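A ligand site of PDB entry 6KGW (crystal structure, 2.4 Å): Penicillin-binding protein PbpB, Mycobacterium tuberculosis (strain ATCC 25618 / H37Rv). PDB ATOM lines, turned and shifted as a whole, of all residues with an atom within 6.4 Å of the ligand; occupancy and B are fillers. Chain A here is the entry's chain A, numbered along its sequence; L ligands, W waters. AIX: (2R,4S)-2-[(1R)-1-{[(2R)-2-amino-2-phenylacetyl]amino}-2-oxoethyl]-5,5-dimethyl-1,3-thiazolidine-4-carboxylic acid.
Residues that only touch the ligand: Gly 268, Ala 307, Gly 477 and Tyr 494.
Hydrophobic or aromatic side chains within 4 Å of the ligand: Ala 307 and Tyr 494.
11 residues have an atom within 4 Å of the ligand: Gly 268, Ser 269, Ala 307, Ser 324, Asn 326, Lys 475, Thr 476, Gly 477, Thr 478, Gln 480 and Tyr 494.
The nearest printed residue that does not touch the ligand is Thr 461 (4.03 Å).
OG of Ser 269 is bonded to C15 of the ligand (1.5 Å).
OG1 of Thr 478 lies within hydrogen-bond range of O2 of the ligand.
The side-chain amide nitrogen (ND2) of Asn 326 is in hydrogen-bond range of an oxygen (O3) of the ligand, 2.5 Å away.
The backbone carbonyl oxygen of Thr 478 lies within hydrogen-bond range of a nitrogen (N1) of the ligand, at 3.1 Å.
NZ of Lys 475 is in salt-bridge range of O1 of the ligand, at 3.5 Å.
N of Thr 478 sits at hydrogen-bond distance from O4 of the ligand, at 2.8 Å.
The backbone NH of Ser 269 sits close to an oxygen (O4) of the ligand, 2.8 Å away.
The side-chain hydroxyl of Thr 476 sits at hydrogen-bond distance from an oxygen (O1) of the ligand (2.7 Å).
A nitrogen (N2) of the ligand lies within hydrogen-bond range of the side-chain amide oxygen (OE1) of Gln 480 (3.1 Å).
The side-chain hydroxyl of Ser 324 is in hydrogen-bond range of a nitrogen (N3) of the ligand.
The backbone carbonyl oxygen of His 305 is in hydrogen-bond range of the side-chain amide nitrogen of Asn 326 (3.3 Å).
OG1 of Thr 476 lies within hydrogen-bond range of OG1 of Thr 461.
The side-chain hydroxyl (OG) of Ser 324 sits at hydrogen-bond distance from the side-chain amino group (NZ) of Lys 475, at 2.7 Å.
The side-chain amino group of Lys 272 is in hydrogen-bond range of the side-chain hydroxyl of Ser 324, at 2.9 Å.
O of Asp 491 lies within hydrogen-bond range of OH of Tyr 494.
The side-chain hydroxyl of Ser 324 sits at hydrogen-bond distance from the side-chain hydroxyl of Ser 269, at 3.2 Å.
The side-chain hydroxyl of Thr 476 lies within hydrogen-bond range of the side-chain amino group of Lys 475, 3.5 Å away.
OG of Ser 269 lies close to NZ of Lys 272.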
ATOM      1  N   PRO A 267      14.273   8.768  11.273  1.00  0.00           N
ATOM      2  CA  PRO A 267      14.713   8.037  10.089  1.00  0.00           C
ATOM      3  C   PRO A 267      15.943   7.149  10.296  1.00  0.00           C
ATOM      4  O   PRO A 267      16.179   6.253   9.471  1.00  0.00           O
ATOM      5  CB  PRO A 267      15.013   9.161   9.094  1.00  0.00           C
ATOM      6  CG  PRO A 267      15.532  10.278  10.021  1.00  0.00           C
ATOM      7  CD  PRO A 267      14.644  10.190  11.235  1.00  0.00           C
ATOM      8  N   GLY A 268      16.742   7.381  11.335  1.00  0.00           N
ATOM      9  CA  GLY A 268      17.998   6.663  11.439  1.00  0.00           C
ATOM     10  C   GLY A 268      18.857   6.875  10.198  1.00  0.00           C
ATOM     11  O   GLY A 268      18.883   7.955   9.614  1.00  0.00           O
ATOM     12  N   SER A 269      19.483   5.787   9.745  1.00  0.00           N
ATOM     13  CA  SER A 269      20.553   5.864   8.760  1.00  0.00           C
ATOM     14  C   SER A 269      20.141   6.307   7.353  1.00  0.00           C
ATOM     15  O   SER A 269      21.019   6.698   6.569  1.00  0.00           O
ATOM     16  CB  SER A 269      21.243   4.516   8.691  1.00  0.00           C
ATOM     17  OG  SER A 269      22.102   4.421   9.780  1.00  0.00           O
ATOM     18  N   VAL A 270      18.856   6.253   6.974  1.00  0.00           N
ATOM     19  CA  VAL A 270      18.543   6.837   5.675  1.00  0.00           C
ATOM     20  C   VAL A 270      18.841   8.324   5.663  1.00  0.00           C
ATOM     21  O   VAL A 270      19.103   8.894   4.601  1.00  0.00           O
ATOM     22  CB  VAL A 270      17.088   6.621   5.205  1.00  0.00           C
ATOM     23  CG1 VAL A 270      16.930   5.219   4.703  1.00  0.00           C
ATOM     24  CG2 VAL A 270      16.100   6.976   6.324  1.00  0.00           C
ATOM     25  N   LYS A 272      21.495   9.610   6.308  1.00  0.00           N
ATOM     26  CA  LYS A 272      22.900   9.885   6.053  1.00  0.00           C
ATOM     27  C   LYS A 272      23.151  10.508   4.678  1.00  0.00           C
ATOM     28  O   LYS A 272      24.246  11.009   4.439  1.00  0.00           O
ATOM     29  CB  LYS A 272      23.718   8.614   6.233  1.00  0.00           C
ATOM     30  CG  LYS A 272      23.832   8.185   7.685  1.00  0.00           C
ATOM     31  CD  LYS A 272      24.703   6.961   7.842  1.00  0.00           C
ATOM     32  CE  LYS A 272      24.629   6.406   9.271  1.00  0.00           C
ATOM     33  NZ  LYS A 272      25.460   5.178   9.404  1.00  0.00           N
ATOM     34  N   HIS A 305      28.548   4.400  18.792  1.00  0.00           N
ATOM     35  CA  HIS A 305      29.131   3.118  18.430  1.00  0.00           C
ATOM     36  C   HIS A 305      28.618   2.671  17.074  1.00  0.00           C
ATOM     37  O   HIS A 305      27.499   3.017  16.665  1.00  0.00           O
ATOM     38  CB  HIS A 305      28.850   2.028  19.528  1.00  0.00           C
ATOM     39  CG  HIS A 305      27.414   1.905  19.969  1.00  0.00           C
ATOM     40  ND1 HIS A 305      26.610   2.986  20.286  1.00  0.00           N
ATOM     41  CD2 HIS A 305      26.646   0.805  20.209  1.00  0.00           C
ATOM     42  CE1 HIS A 305      25.414   2.566  20.671  1.00  0.00           C
ATOM     43  NE2 HIS A 305      25.411   1.249  20.638  1.00  0.00           N
ATOM     44  N   ASP A 306      29.452   1.936  16.343  1.00  0.00           N
ATOM     45  CA  ASP A 306      29.000   1.307  15.109  1.00  0.00           C
ATOM     46  C   ASP A 306      28.273  -0.007  15.419  1.00  0.00           C
ATOM     47  O   ASP A 306      28.533  -0.663  16.419  1.00  0.00           O
ATOM     48  CB  ASP A 306      30.177   1.077  14.176  1.00  0.00           C
ATOM     49  CG  ASP A 306      30.571   2.336  13.387  1.00  0.00           C
ATOM     50  OD1 ASP A 306      29.790   3.326  13.424  1.00  0.00           O
ATOM     51  OD2 ASP A 306      31.627   2.322  12.711  1.00  0.00           O
ATOM     52  N   ALA A 307      27.337  -0.376  14.537  1.00  0.00           N
ATOM     53  CA  ALA A 307      26.512  -1.567  14.772  1.00  0.00           C
ATOM     54  C   ALA A 307      27.320  -2.848  14.882  1.00  0.00           C
ATOM     55  O   ALA A 307      26.745  -3.891  15.216  1.00  0.00           O
ATOM     56  CB  ALA A 307      25.466  -1.732  13.679  1.00  0.00           C
ATOM     57  N   TRP A 308      28.610  -2.814  14.591  1.00  0.00           N
ATOM     58  CA  TRP A 308      29.511  -3.933  14.803  1.00  0.00           C
ATOM     59  C   TRP A 308      30.742  -3.419  15.531  1.00  0.00           C
ATOM     60  O   TRP A 308      31.130  -2.262  15.363  1.00  0.00           O
ATOM     61  CB  TRP A 308      29.879  -4.626  13.484  1.00  0.00           C
ATOM     62  CG  TRP A 308      30.625  -3.771  12.453  1.00  0.00           C
ATOM     63  CD1 TRP A 308      31.923  -3.917  12.063  1.00  0.00           C
ATOM     64  CD2 TRP A 308      30.093  -2.689  11.655  1.00  0.00           C
ATOM     65  NE1 TRP A 308      32.247  -2.996  11.097  1.00  0.00           N
ATOM     66  CE2 TRP A 308      31.145  -2.225  10.833  1.00  0.00           C
ATOM     67  CE3 TRP A 308      28.853  -2.055  11.582  1.00  0.00           C
ATOM     68  CZ2 TRP A 308      30.978  -1.167   9.928  1.00  0.00           C
ATOM     69  CZ3 TRP A 308      28.680  -0.989  10.689  1.00  0.00           C
ATOM     70  CH2 TRP A 308      29.748  -0.558   9.885  1.00  0.00           C
ATOM     71  N   LYS A 323      28.520   0.870   4.210  1.00  0.00           N
ATOM     72  CA  LYS A 323      28.462   0.004   5.376  1.00  0.00           C
ATOM     73  C   LYS A 323      27.693   0.623   6.527  1.00  0.00           C
ATOM     74  O   LYS A 323      27.379  -0.069   7.498  1.00  0.00           O
ATOM     75  CB  LYS A 323      29.876  -0.389   5.839  1.00  0.00           C
ATOM     76  CG  LYS A 323      30.542  -1.436   4.987  1.00  0.00           C
ATOM     77  CD  LYS A 323      31.928  -1.801   5.500  1.00  0.00           C
ATOM     78  CE  LYS A 323      32.663  -2.737   4.548  1.00  0.00           C
ATOM     79  NZ  LYS A 323      31.876  -3.992   4.208  1.00  0.00           N
ATOM     80  N   SER A 324      27.365   1.916   6.409  1.00  0.00           N
ATOM     81  CA  SER A 324      26.592   2.650   7.406  1.00  0.00           C
ATOM     82  C   SER A 324      27.321   2.735   8.754  1.00  0.00           C
ATOM     83  O   SER A 324      26.766   2.427   9.808  1.00  0.00           O
ATOM     84  CB  SER A 324      25.192   2.053   7.561  1.00  0.00           C
ATOM     85  OG  SER A 324      24.245   3.042   7.889  1.00  0.00           O
ATOM     86  N   SER A 325      28.575   3.171   8.705  1.00  0.00           N
ATOM     87  CA  SER A 325      29.320   3.502   9.925  1.00  0.00           C
ATOM     88  C   SER A 325      28.769   4.788  10.548  1.00  0.00           C
ATOM     89  O   SER A 325      28.821   5.855   9.930  1.00  0.00           O
ATOM     90  CB  SER A 325      30.804   3.654   9.594  1.00  0.00           C
ATOM     91  OG  SER A 325      31.523   4.228  10.680  1.00  0.00           O
ATOM     92  N   ASN A 326      28.259   4.696  11.782  1.00  0.00           N
ATOM     93  CA  ASN A 326      27.850   5.893  12.514  1.00  0.00           C
ATOM     94  C   ASN A 326      29.059   6.755  12.839  1.00  0.00           C
ATOM     95  O   ASN A 326      29.043   7.977  12.620  1.00  0.00           O
ATOM     96  CB  ASN A 326      27.104   5.522  13.797  1.00  0.00           C
ATOM     97  CG  ASN A 326      25.724   4.887  13.548  1.00  0.00           C
ATOM     98  OD1 ASN A 326      25.123   5.058  12.490  1.00  0.00           O
ATOM     99  ND2 ASN A 326      25.232   4.164  14.557  1.00  0.00           N
ATOM    100  N   ILE A 382      23.125  10.881  12.015  1.00  0.00           N
ATOM    101  CA  ILE A 382      22.776   9.464  11.908  1.00  0.00           C
ATOM    102  C   ILE A 382      21.267   9.237  11.981  1.00  0.00           C
ATOM    103  O   ILE A 382      20.827   8.093  12.038  1.00  0.00           O
ATOM    104  CB  ILE A 382      23.530   8.632  12.953  1.00  0.00           C
ATOM    105  CG1 ILE A 382      23.105   9.002  14.383  1.00  0.00           C
ATOM    106  CG2 ILE A 382      25.060   8.793  12.779  1.00  0.00           C
ATOM    107  CD1 ILE A 382      23.965   8.337  15.443  1.00  0.00           C
ATOM    108  N   GLN A 384      18.837  10.372  14.295  1.00  0.00           N
ATOM    109  CA  GLN A 384      18.111  10.337  15.557  1.00  0.00           C
ATOM    110  C   GLN A 384      18.022  11.745  16.105  1.00  0.00           C
ATOM    111  O   GLN A 384      18.924  12.562  15.923  1.00  0.00           O
ATOM    112  CB  GLN A 384      18.765   9.389  16.602  1.00  0.00           C
ATOM    113  CG  GLN A 384      18.850   7.878  16.213  1.00  0.00           C
ATOM    114  CD  GLN A 384      17.545   7.016  16.457  1.00  0.00           C
ATOM    115  OE1 GLN A 384      17.611   5.786  16.464  1.00  0.00           O
ATOM    116  NE2 GLN A 384      16.397   7.668  16.628  1.00  0.00           N
ATOM    117  N   THR A 461      25.194  -2.702   3.059  1.00  0.00           N
ATOM    118  CA  THR A 461      24.188  -3.194   3.981  1.00  0.00           C
ATOM    119  C   THR A 461      22.946  -3.730   3.271  1.00  0.00           C
ATOM    120  O   THR A 461      22.153  -4.422   3.914  1.00  0.00           O
ATOM    121  CB  THR A 461      23.755  -2.085   4.952  1.00  0.00           C
ATOM    122  OG1 THR A 461      23.259  -0.969   4.195  1.00  0.00           O
ATOM    123  CG2 THR A 461      24.919  -1.622   5.842  1.00  0.00           C
ATOM    124  N   LYS A 475      19.945   3.553   0.267  1.00  0.00           N
ATOM    125  CA  LYS A 475      20.502   3.598   1.606  1.00  0.00           C
ATOM    126  C   LYS A 475      19.508   2.945   2.562  1.00  0.00           C
ATOM    127  O   LYS A 475      18.306   3.236   2.505  1.00  0.00           O
ATOM    128  CB  LYS A 475      20.810   5.035   2.029  1.00  0.00           C
ATOM    129  CG  LYS A 475      21.331   5.179   3.452  1.00  0.00           C
ATOM    130  CD  LYS A 475      22.748   4.613   3.579  1.00  0.00           C
ATOM    131  CE  LYS A 475      23.221   4.582   5.016  1.00  0.00           C
ATOM    132  NZ  LYS A 475      22.680   3.383   5.720  1.00  0.00           N
ATOM    133  N   THR A 476      20.006   2.067   3.423  1.00  0.00           N
ATOM    134  CA  THR A 476      19.214   1.422   4.464  1.00  0.00           C
ATOM    135  C   THR A 476      19.144   2.305   5.692  1.00  0.00           C
ATOM    136  O   THR A 476      19.948   3.222   5.874  1.00  0.00           O
ATOM    137  CB  THR A 476      19.838   0.082   4.867  1.00  0.00           C
ATOM    138  OG1 THR A 476      21.248   0.264   5.071  1.00  0.00           O
ATOM    139  CG2 THR A 476      19.598  -1.012   3.783  1.00  0.00           C
ATOM    140  N   GLY A 477      18.195   1.988   6.576  1.00  0.00           N
ATOM    141  CA  GLY A 477      18.195   2.568   7.906  1.00  0.00           C
ATOM    142  C   GLY A 477      17.565   1.661   8.940  1.00  0.00           C
ATOM    143  O   GLY A 477      16.673   0.867   8.642  1.00  0.00           O
ATOM    144  N   THR A 478      18.022   1.822  10.181  1.00  0.00           N
ATOM    145  CA  THR A 478      17.489   1.107  11.345  1.00  0.00           C
ATOM    146  C   THR A 478      17.527   2.119  12.496  1.00  0.00           C
ATOM    147  O   THR A 478      18.581   2.335  13.108  1.00  0.00           O
ATOM    148  CB  THR A 478      18.305  -0.138  11.686  1.00  0.00           C
ATOM    149  OG1 THR A 478      18.459  -0.967  10.534  1.00  0.00           O
ATOM    150  CG2 THR A 478      17.636  -0.954  12.780  1.00  0.00           C
ATOM    151  N   ALA A 479      16.389   2.732  12.784  1.00  0.00           N
ATOM    152  CA  ALA A 479      16.284   3.748  13.817  1.00  0.00           C
ATOM    153  C   ALA A 479      15.552   3.178  15.025  1.00  0.00           C
ATOM    154  O   ALA A 479      14.578   2.437  14.880  1.00  0.00           O
ATOM    155  CB  ALA A 479      15.546   4.981  13.305  1.00  0.00           C
ATOM    156  N   GLN A 480      16.014   3.537  16.226  1.00  0.00           N
ATOM    157  CA  GLN A 480      15.356   3.045  17.427  1.00  0.00           C
ATOM    158  C   GLN A 480      14.125   3.884  17.748  1.00  0.00           C
ATOM    159  O   GLN A 480      14.132   5.111  17.616  1.00  0.00           O
ATOM    160  CB  GLN A 480      16.331   3.056  18.592  1.00  0.00           C
ATOM    161  CG  GLN A 480      17.475   2.070  18.430  1.00  0.00           C
ATOM    162  CD  GLN A 480      18.516   2.256  19.498  1.00  0.00           C
ATOM    163  OE1 GLN A 480      19.527   2.969  19.304  1.00  0.00           O
ATOM    164  NE2 GLN A 480      18.298   1.636  20.655  1.00  0.00           N
ATOM    165  N   ASP A 491      15.563  -0.707  22.989  1.00  0.00           N
ATOM    166  CA  ASP A 491      16.767  -1.363  22.490  1.00  0.00           C
ATOM    167  C   ASP A 491      16.507  -2.186  21.248  1.00  0.00           C
ATOM    168  O   ASP A 491      17.381  -2.274  20.385  1.00  0.00           O
ATOM    169  CB  ASP A 491      17.385  -2.250  23.579  1.00  0.00           C
ATOM    170  CG  ASP A 491      17.579  -1.516  24.892  1.00  0.00           C
ATOM    171  OD1 ASP A 491      16.696  -1.635  25.772  1.00  0.00           O
ATOM    172  OD2 ASP A 491      18.597  -0.813  25.044  1.00  0.00           O
ATOM    173  N   TYR A 494      12.387  -1.048  16.224  1.00  0.00           N
ATOM    174  CA  TYR A 494      12.986  -0.208  15.191  1.00  0.00           C
ATOM    175  C   TYR A 494      11.971   0.214  14.141  1.00  0.00           C
ATOM    176  O   TYR A 494      10.971  -0.455  13.895  1.00  0.00           O
ATOM    177  CB  TYR A 494      14.143  -0.931  14.490  1.00  0.00           C
ATOM    178  CG  TYR A 494      15.180  -1.503  15.447  1.00  0.00           C
ATOM    179  CD1 TYR A 494      16.069  -0.670  16.118  1.00  0.00           C
ATOM    180  CD2 TYR A 494      15.276  -2.874  15.660  1.00  0.00           C
ATOM    181  CE1 TYR A 494      17.032  -1.188  16.974  1.00  0.00           C
ATOM    182  CE2 TYR A 494      16.225  -3.407  16.527  1.00  0.00           C
ATOM    183  CZ  TYR A 494      17.099  -2.554  17.180  1.00  0.00           C
ATOM    184  OH  TYR A 494      18.058  -3.066  18.047  1.00  0.00           O
ATOM    185  N   THR A 497      13.861   1.135   7.235  1.00  0.00           N
ATOM    186  CA  THR A 497      13.637   2.164   6.242  1.00  0.00           C
ATOM    187  C   THR A 497      14.603   1.913   5.086  1.00  0.00           C
ATOM    188  O   THR A 497      15.726   1.477   5.312  1.00  0.00           O
ATOM    189  CB  THR A 497      13.819   3.532   6.936  1.00  0.00           C
ATOM    190  OG1 THR A 497      13.187   4.570   6.201  1.00  0.00           O
ATOM    191  CG2 THR A 497      15.243   3.852   7.195  1.00  0.00           C
HETATM  192  C8  AIX L   1      20.114  -1.838  15.371  1.00  0.00           C
HETATM  193  C5  AIX L   1      21.114   0.345  15.401  1.00  0.00           C
HETATM  194  C6  AIX L   1      22.851  -0.597  10.669  1.00  0.00           C
HETATM  195  N1  AIX L   1      21.661   2.362  13.040  1.00  0.00           N
HETATM  196  C2  AIX L   1      21.389  -0.036   8.623  1.00  0.00           C
HETATM  197  N3  AIX L   1      22.511   1.720   9.887  1.00  0.00           N
HETATM  198  C4  AIX L   1      20.984   1.858  15.316  1.00  0.00           C
HETATM  199  C1  AIX L   1      23.911  -1.173   9.737  1.00  0.00           C
HETATM  200  C3  AIX L   1      21.987   2.476  14.332  1.00  0.00           C
HETATM  201  C7  AIX L   1      19.993  -0.458  15.336  1.00  0.00           C
HETATM  202  C9  AIX L   1      21.358  -2.430  15.471  1.00  0.00           C
HETATM  203  C10 AIX L   1      22.475  -1.634  15.548  1.00  0.00           C
HETATM  204  C11 AIX L   1      22.361  -0.252  15.525  1.00  0.00           C
HETATM  205  C12 AIX L   1      21.860   0.408   9.990  1.00  0.00           C
HETATM  206  C13 AIX L   1      23.265   2.037  11.084  1.00  0.00           C
HETATM  207  C14 AIX L   1      22.377   3.005  11.940  1.00  0.00           C
HETATM  208  C15 AIX L   1      21.423   3.704  10.907  1.00  0.00           C
HETATM  209  C16 AIX L   1      22.071  -1.706  11.370  1.00  0.00           C
HETATM  210  N2  AIX L   1      21.057   2.481  16.652  1.00  0.00           N
HETATM  211  O1  AIX L   1      22.005   0.623   7.682  1.00  0.00           O
HETATM  212  O2  AIX L   1      20.539  -0.901   8.415  1.00  0.00           O
HETATM  213  O3  AIX L   1      23.011   3.038  14.725  1.00  0.00           O
HETATM  214  O4  AIX L   1      20.331   3.260  10.641  1.00  0.00           O
HETATM  215  S1  AIX L   1      23.666   0.460  11.934  1.00  0.00           S
HETATM  216  O   HOH W   1      23.700   2.740  17.926  1.00  0.00           O
